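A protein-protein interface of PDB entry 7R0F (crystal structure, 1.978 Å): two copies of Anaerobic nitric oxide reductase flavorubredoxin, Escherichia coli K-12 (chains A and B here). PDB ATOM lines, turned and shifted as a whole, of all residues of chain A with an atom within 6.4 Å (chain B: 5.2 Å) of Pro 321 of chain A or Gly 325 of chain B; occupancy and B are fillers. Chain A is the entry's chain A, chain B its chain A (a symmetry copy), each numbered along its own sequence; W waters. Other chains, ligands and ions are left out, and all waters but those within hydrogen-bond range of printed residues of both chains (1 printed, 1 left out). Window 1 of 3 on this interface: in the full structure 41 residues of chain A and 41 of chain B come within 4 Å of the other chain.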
ATOM      1  N   ASP A 259       9.486 -19.201  -5.578  1.00  0.00           N
ATOM      2  CA  ASP A 259      10.161 -20.200  -6.394  1.00  0.00           C
ATOM      3  C   ASP A 259      11.574 -20.376  -5.852  1.00  0.00           C
ATOM      4  O   ASP A 259      12.160 -19.436  -5.313  1.00  0.00           O
ATOM      5  CB  ASP A 259      10.187 -19.800  -7.869  1.00  0.00           C
ATOM      6  CG  ASP A 259      10.264 -21.004  -8.796  1.00  0.00           C
ATOM      7  OD1 ASP A 259      10.641 -22.098  -8.326  1.00  0.00           O
ATOM      8  OD2 ASP A 259       9.938 -20.858  -9.993  1.00  0.00           O
ATOM      9  N   THR A 312      11.815 -15.288  -3.731  1.00  0.00           N
ATOM     10  CA  THR A 312      12.575 -15.623  -4.924  1.00  0.00           C
ATOM     11  C   THR A 312      14.064 -15.620  -4.617  1.00  0.00           C
ATOM     12  O   THR A 312      14.543 -14.823  -3.809  1.00  0.00           O
ATOM     13  CB  THR A 312      12.290 -14.642  -6.085  1.00  0.00           C
ATOM     14  OG1 THR A 312      13.018 -15.053  -7.250  1.00  0.00           O
ATOM     15  CG2 THR A 312      12.696 -13.222  -5.713  1.00  0.00           C
ATOM     16  N   MET A 315      18.755 -15.219  -9.548  1.00  0.00           N
ATOM     17  CA  MET A 315      19.239 -16.018 -10.661  1.00  0.00           C
ATOM     18  C   MET A 315      19.661 -15.098 -11.797  1.00  0.00           C
ATOM     19  O   MET A 315      18.820 -14.439 -12.409  1.00  0.00           O
ATOM     20  CB  MET A 315      18.162 -16.997 -11.127  1.00  0.00           C
ATOM     21  CG  MET A 315      18.555 -17.851 -12.320  1.00  0.00           C
ATOM     22  SD  MET A 315      17.162 -18.824 -12.931  1.00  0.00           S
ATOM     23  CE  MET A 315      17.891 -19.590 -14.377  1.00  0.00           C
ATOM     24  N   MET A 319      15.179 -12.008 -10.853  1.00  0.00           N
ATOM     25  CA  MET A 319      14.349 -12.938 -10.098  1.00  0.00           C
ATOM     26  C   MET A 319      13.977 -14.147 -10.949  1.00  0.00           C
ATOM     27  O   MET A 319      14.144 -14.133 -12.169  1.00  0.00           O
ATOM     28  CB  MET A 319      13.084 -12.242  -9.589  1.00  0.00           C
ATOM     29  CG  MET A 319      12.040 -11.982 -10.663  1.00  0.00           C
ATOM     30  SD  MET A 319      10.619 -11.053 -10.047  1.00  0.00           S
ATOM     31  CE  MET A 319      11.301  -9.402  -9.976  1.00  0.00           C
ATOM     32  N   MET A 320      13.475 -15.193 -10.299  1.00  0.00           N
ATOM     33  CA  MET A 320      13.042 -16.388 -11.008  1.00  0.00           C
ATOM     34  C   MET A 320      11.810 -16.076 -11.857  1.00  0.00           C
ATOM     35  O   MET A 320      10.888 -15.404 -11.393  1.00  0.00           O
ATOM     36  CB  MET A 320      12.760 -17.524 -10.023  1.00  0.00           C
ATOM     37  CG  MET A 320      13.975 -17.913  -9.191  1.00  0.00           C
ATOM     38  SD  MET A 320      13.788 -19.489  -8.339  1.00  0.00           S
ATOM     39  CE  MET A 320      13.581 -20.596  -9.732  1.00  0.00           C
ATOM     40  N   PRO A 321      11.798 -16.563 -13.108  1.00  0.00           N
ATOM     41  CA  PRO A 321      10.797 -16.221 -14.130  1.00  0.00           C
ATOM     42  C   PRO A 321       9.344 -16.501 -13.744  1.00  0.00           C
ATOM     43  O   PRO A 321       8.477 -15.701 -14.094  1.00  0.00           O
ATOM     44  CB  PRO A 321      11.201 -17.095 -15.325  1.00  0.00           C
ATOM     45  CG  PRO A 321      12.094 -18.138 -14.771  1.00  0.00           C
ATOM     46  CD  PRO A 321      12.802 -17.505 -13.625  1.00  0.00           C
ATOM     47  N   LYS A 322       9.073 -17.605 -13.057  1.00  0.00           N
ATOM     48  CA  LYS A 322       7.694 -17.931 -12.696  1.00  0.00           C
ATOM     49  C   LYS A 322       7.144 -16.925 -11.695  1.00  0.00           C
ATOM     50  O   LYS A 322       5.942 -16.654 -11.671  1.00  0.00           O
ATOM     51  CB  LYS A 322       7.591 -19.348 -12.131  1.00  0.00           C
ATOM     52  CG  LYS A 322       7.671 -20.441 -13.181  1.00  0.00           C
ATOM     53  CD  LYS A 322       7.377 -21.804 -12.578  1.00  0.00           C
ATOM     54  CE  LYS A 322       7.594 -22.918 -13.589  1.00  0.00           C
ATOM     55  NZ  LYS A 322       9.014 -23.006 -14.022  1.00  0.00           N
ATOM     56  N   ILE A 323       8.028 -16.372 -10.873  1.00  0.00           N
ATOM     57  CA  ILE A 323       7.648 -15.307  -9.954  1.00  0.00           C
ATOM     58  C   ILE A 323       7.381 -14.029 -10.742  1.00  0.00           C
ATOM     59  O   ILE A 323       6.390 -13.341 -10.509  1.00  0.00           O
ATOM     60  CB  ILE A 323       8.732 -15.056  -8.890  1.00  0.00           C
ATOM     61  CG1 ILE A 323       8.842 -16.260  -7.954  1.00  0.00           C
ATOM     62  CG2 ILE A 323       8.421 -13.800  -8.091  1.00  0.00           C
ATOM     63  CD1 ILE A 323       7.596 -16.502  -7.124  1.00  0.00           C
ATOM     64  N   ALA A 324       8.273 -13.723 -11.681  1.00  0.00           N
ATOM     65  CA  ALA A 324       8.115 -12.558 -12.544  1.00  0.00           C
ATOM     66  C   ALA A 324       6.823 -12.647 -13.348  1.00  0.00           C
ATOM     67  O   ALA A 324       6.123 -11.652 -13.529  1.00  0.00           O
ATOM     68  CB  ALA A 324       9.309 -12.423 -13.475  1.00  0.00           C
ATOM     69  N   GLY A 325       6.511 -13.848 -13.826  1.00  0.00           N
ATOM     70  CA  GLY A 325       5.282 -14.079 -14.559  1.00  0.00           C
ATOM     71  C   GLY A 325       4.056 -13.861 -13.692  1.00  0.00           C
ATOM     72  O   GLY A 325       3.100 -13.209 -14.105  1.00  0.00           O
ATOM     73  N   LEU A 326       4.088 -14.408 -12.481  1.00  0.00           N
ATOM     74  CA  LEU A 326       2.954 -14.307 -11.569  1.00  0.00           C
ATOM     75  C   LEU A 326       2.703 -12.865 -11.128  1.00  0.00           C
ATOM     76  O   LEU A 326       1.556 -12.428 -11.053  1.00  0.00           O
ATOM     77  CB  LEU A 326       3.175 -15.202 -10.348  1.00  0.00           C
ATOM     78  CG  LEU A 326       1.944 -15.462  -9.478  1.00  0.00           C
ATOM     79  CD1 LEU A 326       0.732 -15.774 -10.344  1.00  0.00           C
ATOM     80  CD2 LEU A 326       2.212 -16.604  -8.514  1.00  0.00           C
ATOM     81  N   GLU A 328       3.467 -10.193 -12.787  1.00  0.00           N
ATOM     82  CA  GLU A 328       2.916  -9.513 -13.955  1.00  0.00           C
ATOM     83  C   GLU A 328       1.403  -9.696 -14.036  1.00  0.00           C
ATOM     84  O   GLU A 328       0.668  -8.743 -14.295  1.00  0.00           O
ATOM     85  CB  GLU A 328       3.574 -10.023 -15.239  1.00  0.00           C
ATOM     86  CG  GLU A 328       2.986  -9.443 -16.522  1.00  0.00           C
ATOM     87  CD  GLU A 328       3.464  -8.028 -16.815  1.00  0.00           C
ATOM     88  OE1 GLU A 328       4.216  -7.462 -15.995  1.00  0.00           O
ATOM     89  OE2 GLU A 328       3.088  -7.483 -17.875  1.00  0.00           O
ATOM     90  N   GLU B  26      14.005 -24.799 -13.794  1.00  0.00           N
ATOM     91  CA  GLU B  26      14.486 -23.840 -14.782  1.00  0.00           C
ATOM     92  C   GLU B  26      15.338 -24.478 -15.871  1.00  0.00           C
ATOM     93  O   GLU B  26      15.469 -23.927 -16.965  1.00  0.00           O
ATOM     94  CB  GLU B  26      15.276 -22.727 -14.091  1.00  0.00           C
ATOM     95  CG  GLU B  26      14.427 -21.844 -13.194  1.00  0.00           C
ATOM     96  CD  GLU B  26      13.207 -21.301 -13.912  1.00  0.00           C
ATOM     97  OE1 GLU B  26      13.323 -20.964 -15.109  1.00  0.00           O
ATOM     98  OE2 GLU B  26      12.131 -21.216 -13.281  1.00  0.00           O
ATOM     99  N   LYS B 295      10.968 -24.691 -22.491  1.00  0.00           N
ATOM    100  CA  LYS B 295      11.512 -23.357 -22.271  1.00  0.00           C
ATOM    101  C   LYS B 295      12.990 -23.272 -22.642  1.00  0.00           C
ATOM    102  O   LYS B 295      13.437 -22.284 -23.222  1.00  0.00           O
ATOM    103  CB  LYS B 295      11.324 -22.939 -20.811  1.00  0.00           C
ATOM    104  CG  LYS B 295      11.725 -21.502 -20.533  1.00  0.00           C
ATOM    105  CD  LYS B 295      12.075 -21.289 -19.071  1.00  0.00           C
ATOM    106  CE  LYS B 295      13.348 -22.030 -18.702  1.00  0.00           C
ATOM    107  NZ  LYS B 295      13.882 -21.596 -17.383  1.00  0.00           N
ATOM    108  N   PRO B 321       1.662 -13.748 -18.761  1.00  0.00           N
ATOM    109  CA  PRO B 321       2.681 -14.020 -17.735  1.00  0.00           C
ATOM    110  C   PRO B 321       3.850 -14.896 -18.187  1.00  0.00           C
ATOM    111  O   PRO B 321       4.978 -14.629 -17.776  1.00  0.00           O
ATOM    112  CB  PRO B 321       1.887 -14.732 -16.631  1.00  0.00           C
ATOM    113  CG  PRO B 321       0.628 -15.177 -17.270  1.00  0.00           C
ATOM    114  CD  PRO B 321       0.323 -14.169 -18.322  1.00  0.00           C
ATOM    115  N   LYS B 322       3.598 -15.919 -18.996  1.00  0.00           N
ATOM    116  CA  LYS B 322       4.679 -16.803 -19.427  1.00  0.00           C
ATOM    117  C   LYS B 322       5.658 -16.064 -20.327  1.00  0.00           C
ATOM    118  O   LYS B 322       6.850 -16.378 -20.354  1.00  0.00           O
ATOM    119  CB  LYS B 322       4.131 -18.037 -20.145  1.00  0.00           C
ATOM    120  CG  LYS B 322       3.527 -19.075 -19.217  1.00  0.00           C
ATOM    121  CD  LYS B 322       3.174 -20.346 -19.972  1.00  0.00           C
ATOM    122  CE  LYS B 322       2.441 -21.336 -19.082  1.00  0.00           C
ATOM    123  NZ  LYS B 322       1.129 -20.804 -18.623  1.00  0.00           N
ATOM    124  N   ILE B 323       5.152 -15.079 -21.062  1.00  0.00           N
ATOM    125  CA  ILE B 323       6.006 -14.218 -21.869  1.00  0.00           C
ATOM    126  C   ILE B 323       6.811 -13.301 -20.955  1.00  0.00           C
ATOM    127  O   ILE B 323       8.015 -13.129 -21.139  1.00  0.00           O
ATOM    128  CB  ILE B 323       5.189 -13.381 -22.871  1.00  0.00           C
ATOM    129  CG1 ILE B 323       4.560 -14.289 -23.929  1.00  0.00           C
ATOM    130  CG2 ILE B 323       6.066 -12.333 -23.537  1.00  0.00           C
ATOM    131  CD1 ILE B 323       5.575 -14.988 -24.813  1.00  0.00           C
ATOM    132  N   ALA B 324       6.137 -12.722 -19.965  1.00  0.00           N
ATOM    133  CA  ALA B 324       6.793 -11.863 -18.986  1.00  0.00           C
ATOM    134  C   ALA B 324       7.876 -12.625 -18.231  1.00  0.00           C
ATOM    135  O   ALA B 324       8.951 -12.092 -17.963  1.00  0.00           O
ATOM    136  CB  ALA B 324       5.772 -11.293 -18.015  1.00  0.00           C
ATOM    137  N   GLY B 325       7.584 -13.878 -17.894  1.00  0.00           N
ATOM    138  CA  GLY B 325       8.547 -14.728 -17.224  1.00  0.00           C
ATOM    139  C   GLY B 325       9.758 -15.009 -18.094  1.00  0.00           C
ATOM    140  O   GLY B 325      10.896 -14.922 -17.639  1.00  0.00           O
ATOM    141  N   LEU B 326       9.509 -15.344 -19.356  1.00  0.00           N
ATOM    142  CA  LEU B 326      10.585 -15.681 -20.281  1.00  0.00           C
ATOM    143  C   LEU B 326      11.486 -14.480 -20.570  1.00  0.00           C
ATOM    144  O   LEU B 326      12.707 -14.617 -20.628  1.00  0.00           O
ATOM    145  CB  LEU B 326      10.009 -16.235 -21.586  1.00  0.00           C
ATOM    146  CG  LEU B 326      11.002 -16.939 -22.511  1.00  0.00           C
ATOM    147  CD1 LEU B 326      11.910 -17.866 -21.716  1.00  0.00           C
ATOM    148  CD2 LEU B 326      10.263 -17.715 -23.585  1.00  0.00           C
ATOM    149  N   VAL B 327      10.883 -13.308 -20.746  1.00  0.00           N
ATOM    150  CA  VAL B 327      11.642 -12.088 -21.013  1.00  0.00           C
ATOM    151  C   VAL B 327      12.518 -11.722 -19.813  1.00  0.00           C
ATOM    152  O   VAL B 327      13.645 -11.252 -19.976  1.00  0.00           O
ATOM    153  CB  VAL B 327      10.709 -10.907 -21.365  1.00  0.00           C
ATOM    154  CG1 VAL B 327      11.496  -9.611 -21.485  1.00  0.00           C
ATOM    155  CG2 VAL B 327       9.964 -11.193 -22.656  1.00  0.00           C
ATOM    156  N   GLU B 328      11.999 -11.954 -18.612  1.00  0.00           N
ATOM    157  CA  GLU B 328      12.771 -11.737 -17.393  1.00  0.00           C
ATOM    158  C   GLU B 328      14.025 -12.606 -17.373  1.00  0.00           C
ATOM    159  O   GLU B 328      15.110 -12.135 -17.032  1.00  0.00           O
ATOM    160  CB  GLU B 328      11.917 -12.021 -16.154  1.00  0.00           C
ATOM    161  CG  GLU B 328      12.673 -11.920 -14.832  1.00  0.00           C
ATOM    162  CD  GLU B 328      12.895 -10.486 -14.375  1.00  0.00           C
ATOM    163  OE1 GLU B 328      12.511  -9.551 -15.109  1.00  0.00           O
ATOM    164  OE2 GLU B 328      13.452 -10.294 -13.273  1.00  0.00           O
ATOM    165  N   GLU B 329      13.872 -13.873 -17.741  1.00  0.00           N
ATOM    166  CA  GLU B 329      15.003 -14.794 -17.767  1.00  0.00           C
ATOM    167  C   GLU B 329      16.017 -14.387 -18.832  1.00  0.00           C
ATOM    168  O   GLU B 329      17.226 -14.480 -18.619  1.00  0.00           O
ATOM    169  CB  GLU B 329      14.530 -16.226 -18.017  1.00  0.00           C
ATOM    170  CG  GLU B 329      15.651 -17.253 -17.991  1.00  0.00           C
ATOM    171  CD  GLU B 329      15.136 -18.676 -17.978  1.00  0.00           C
ATOM    172  OE1 GLU B 329      13.906 -18.861 -18.086  1.00  0.00           O
ATOM    173  OE2 GLU B 329      15.959 -19.608 -17.858  1.00  0.00           O
HETATM  174  O   HOH W   1      11.747 -23.153 -10.931  1.00  0.00           O
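OE2 of Glu 328 of chain B lies close to N of Met 319 of chain A (3.4 Å). NZ of Lys 322 of chain A is in salt-bridge range of OE2 of Glu 26 of chain B, at 3.7 Å.
The backbone NH (N) of Met 320 of chain A lies within hydrogen-bond range of the side-chain hydroxyl (OG1) of Thr 312 of chain A (3.1 Å). The side-chain carboxylate of Glu 26 of chain B lies within salt-bridge range of the side-chain amino group of Lys 295 of chain B, at 2.4 Å. The side-chain amino group of Lys 295 of chain B lies within salt-bridge range of the side-chain carboxylate of Glu 329 of chain B (2.8 Å).
Asp 259 of chain A touches Glu 26 of chain B. Met 315 of chain A touches Glu 329 of chain B. Glu 26 of chain B touches Met 320 of chain A (CG to CE, 3.8 Å). CG of Pro 321 of chain A touches OE1 of Glu 26 of chain B (3.1 Å). CB of Pro 321 of chain A touches O of Gly 325 of chain B (3.2 Å). Pro 321 of chain A touches Glu 329 of chain B. CB of Ala 324 of chain A touches CG of Glu 328 of chain B, at 3.7 Å. Gly 325 of chain A touches Pro 321 of chain B. Ala 324 of chain B touches Glu 328 of chain A (CB to CG, 3.7 Å).
Of chain B, only Glu 26, Gly 325 and Glu 329 come within 4 Å of Pro 321 of chain A. Printed residues of chain B within 4 Å of Lys 322 of chain A: Glu 26 (3.7 Å). Of the printed residues of chain B, Ala 324 of chain A touches Glu 328. Printed residues of chain B within 4 Å of Glu 328 of chain A: Ala 324. Of the printed residues of chain A, Glu 26 of chain B touches Asp 259, Met 320, Pro 321 and Lys 322. Of chain A, only Pro 321 (3.2 Å) comes within 4 Å of Gly 325 of chain B. The nearest printed residue of chain B that does not touch Pro 321 of chain A is Lys 295 of chain B (4.7 Å). The nearest residue of chain A that does not touch Gly 325 of chain B is Gly 325 of chain A (4.1 Å). The nearest printed residue of chain B that does not touch Gly 325 of chain A is Gly 325 of chain B (4.1 Å).
Of the 11 printed residues of chain B, 6 touch a printed residue of chain A. Of the 12 printed residues of chain A, 9 touch a printed residue of chain B. Hydrophobic or aromatic side chains of chain A within 4 Å of the printed part of chain B: Met 315, Met 319, Met 320, Pro 321 and Ala 324.
Pro 321 of chain A touches Gly 325 of chain B, and with the chains exchanged Gly 325 of chain A touches Pro 321 of chain B. Ala 324 of chain A touches Glu 328 of chain B, and with the chains exchanged Glu 328 of chain A touches Ala 324 of chain B. 7 positions are printed for both chains. Of the 11 pairs that touch across the chains among the printed residues, 4 have their exchanged pair printed and touching as well.
Water W1 bridges the side-chain carboxylate of Asp 259 of chain A (3.0 Å) and the side-chain carboxylate of Glu 26 of chain B (3.1 Å).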
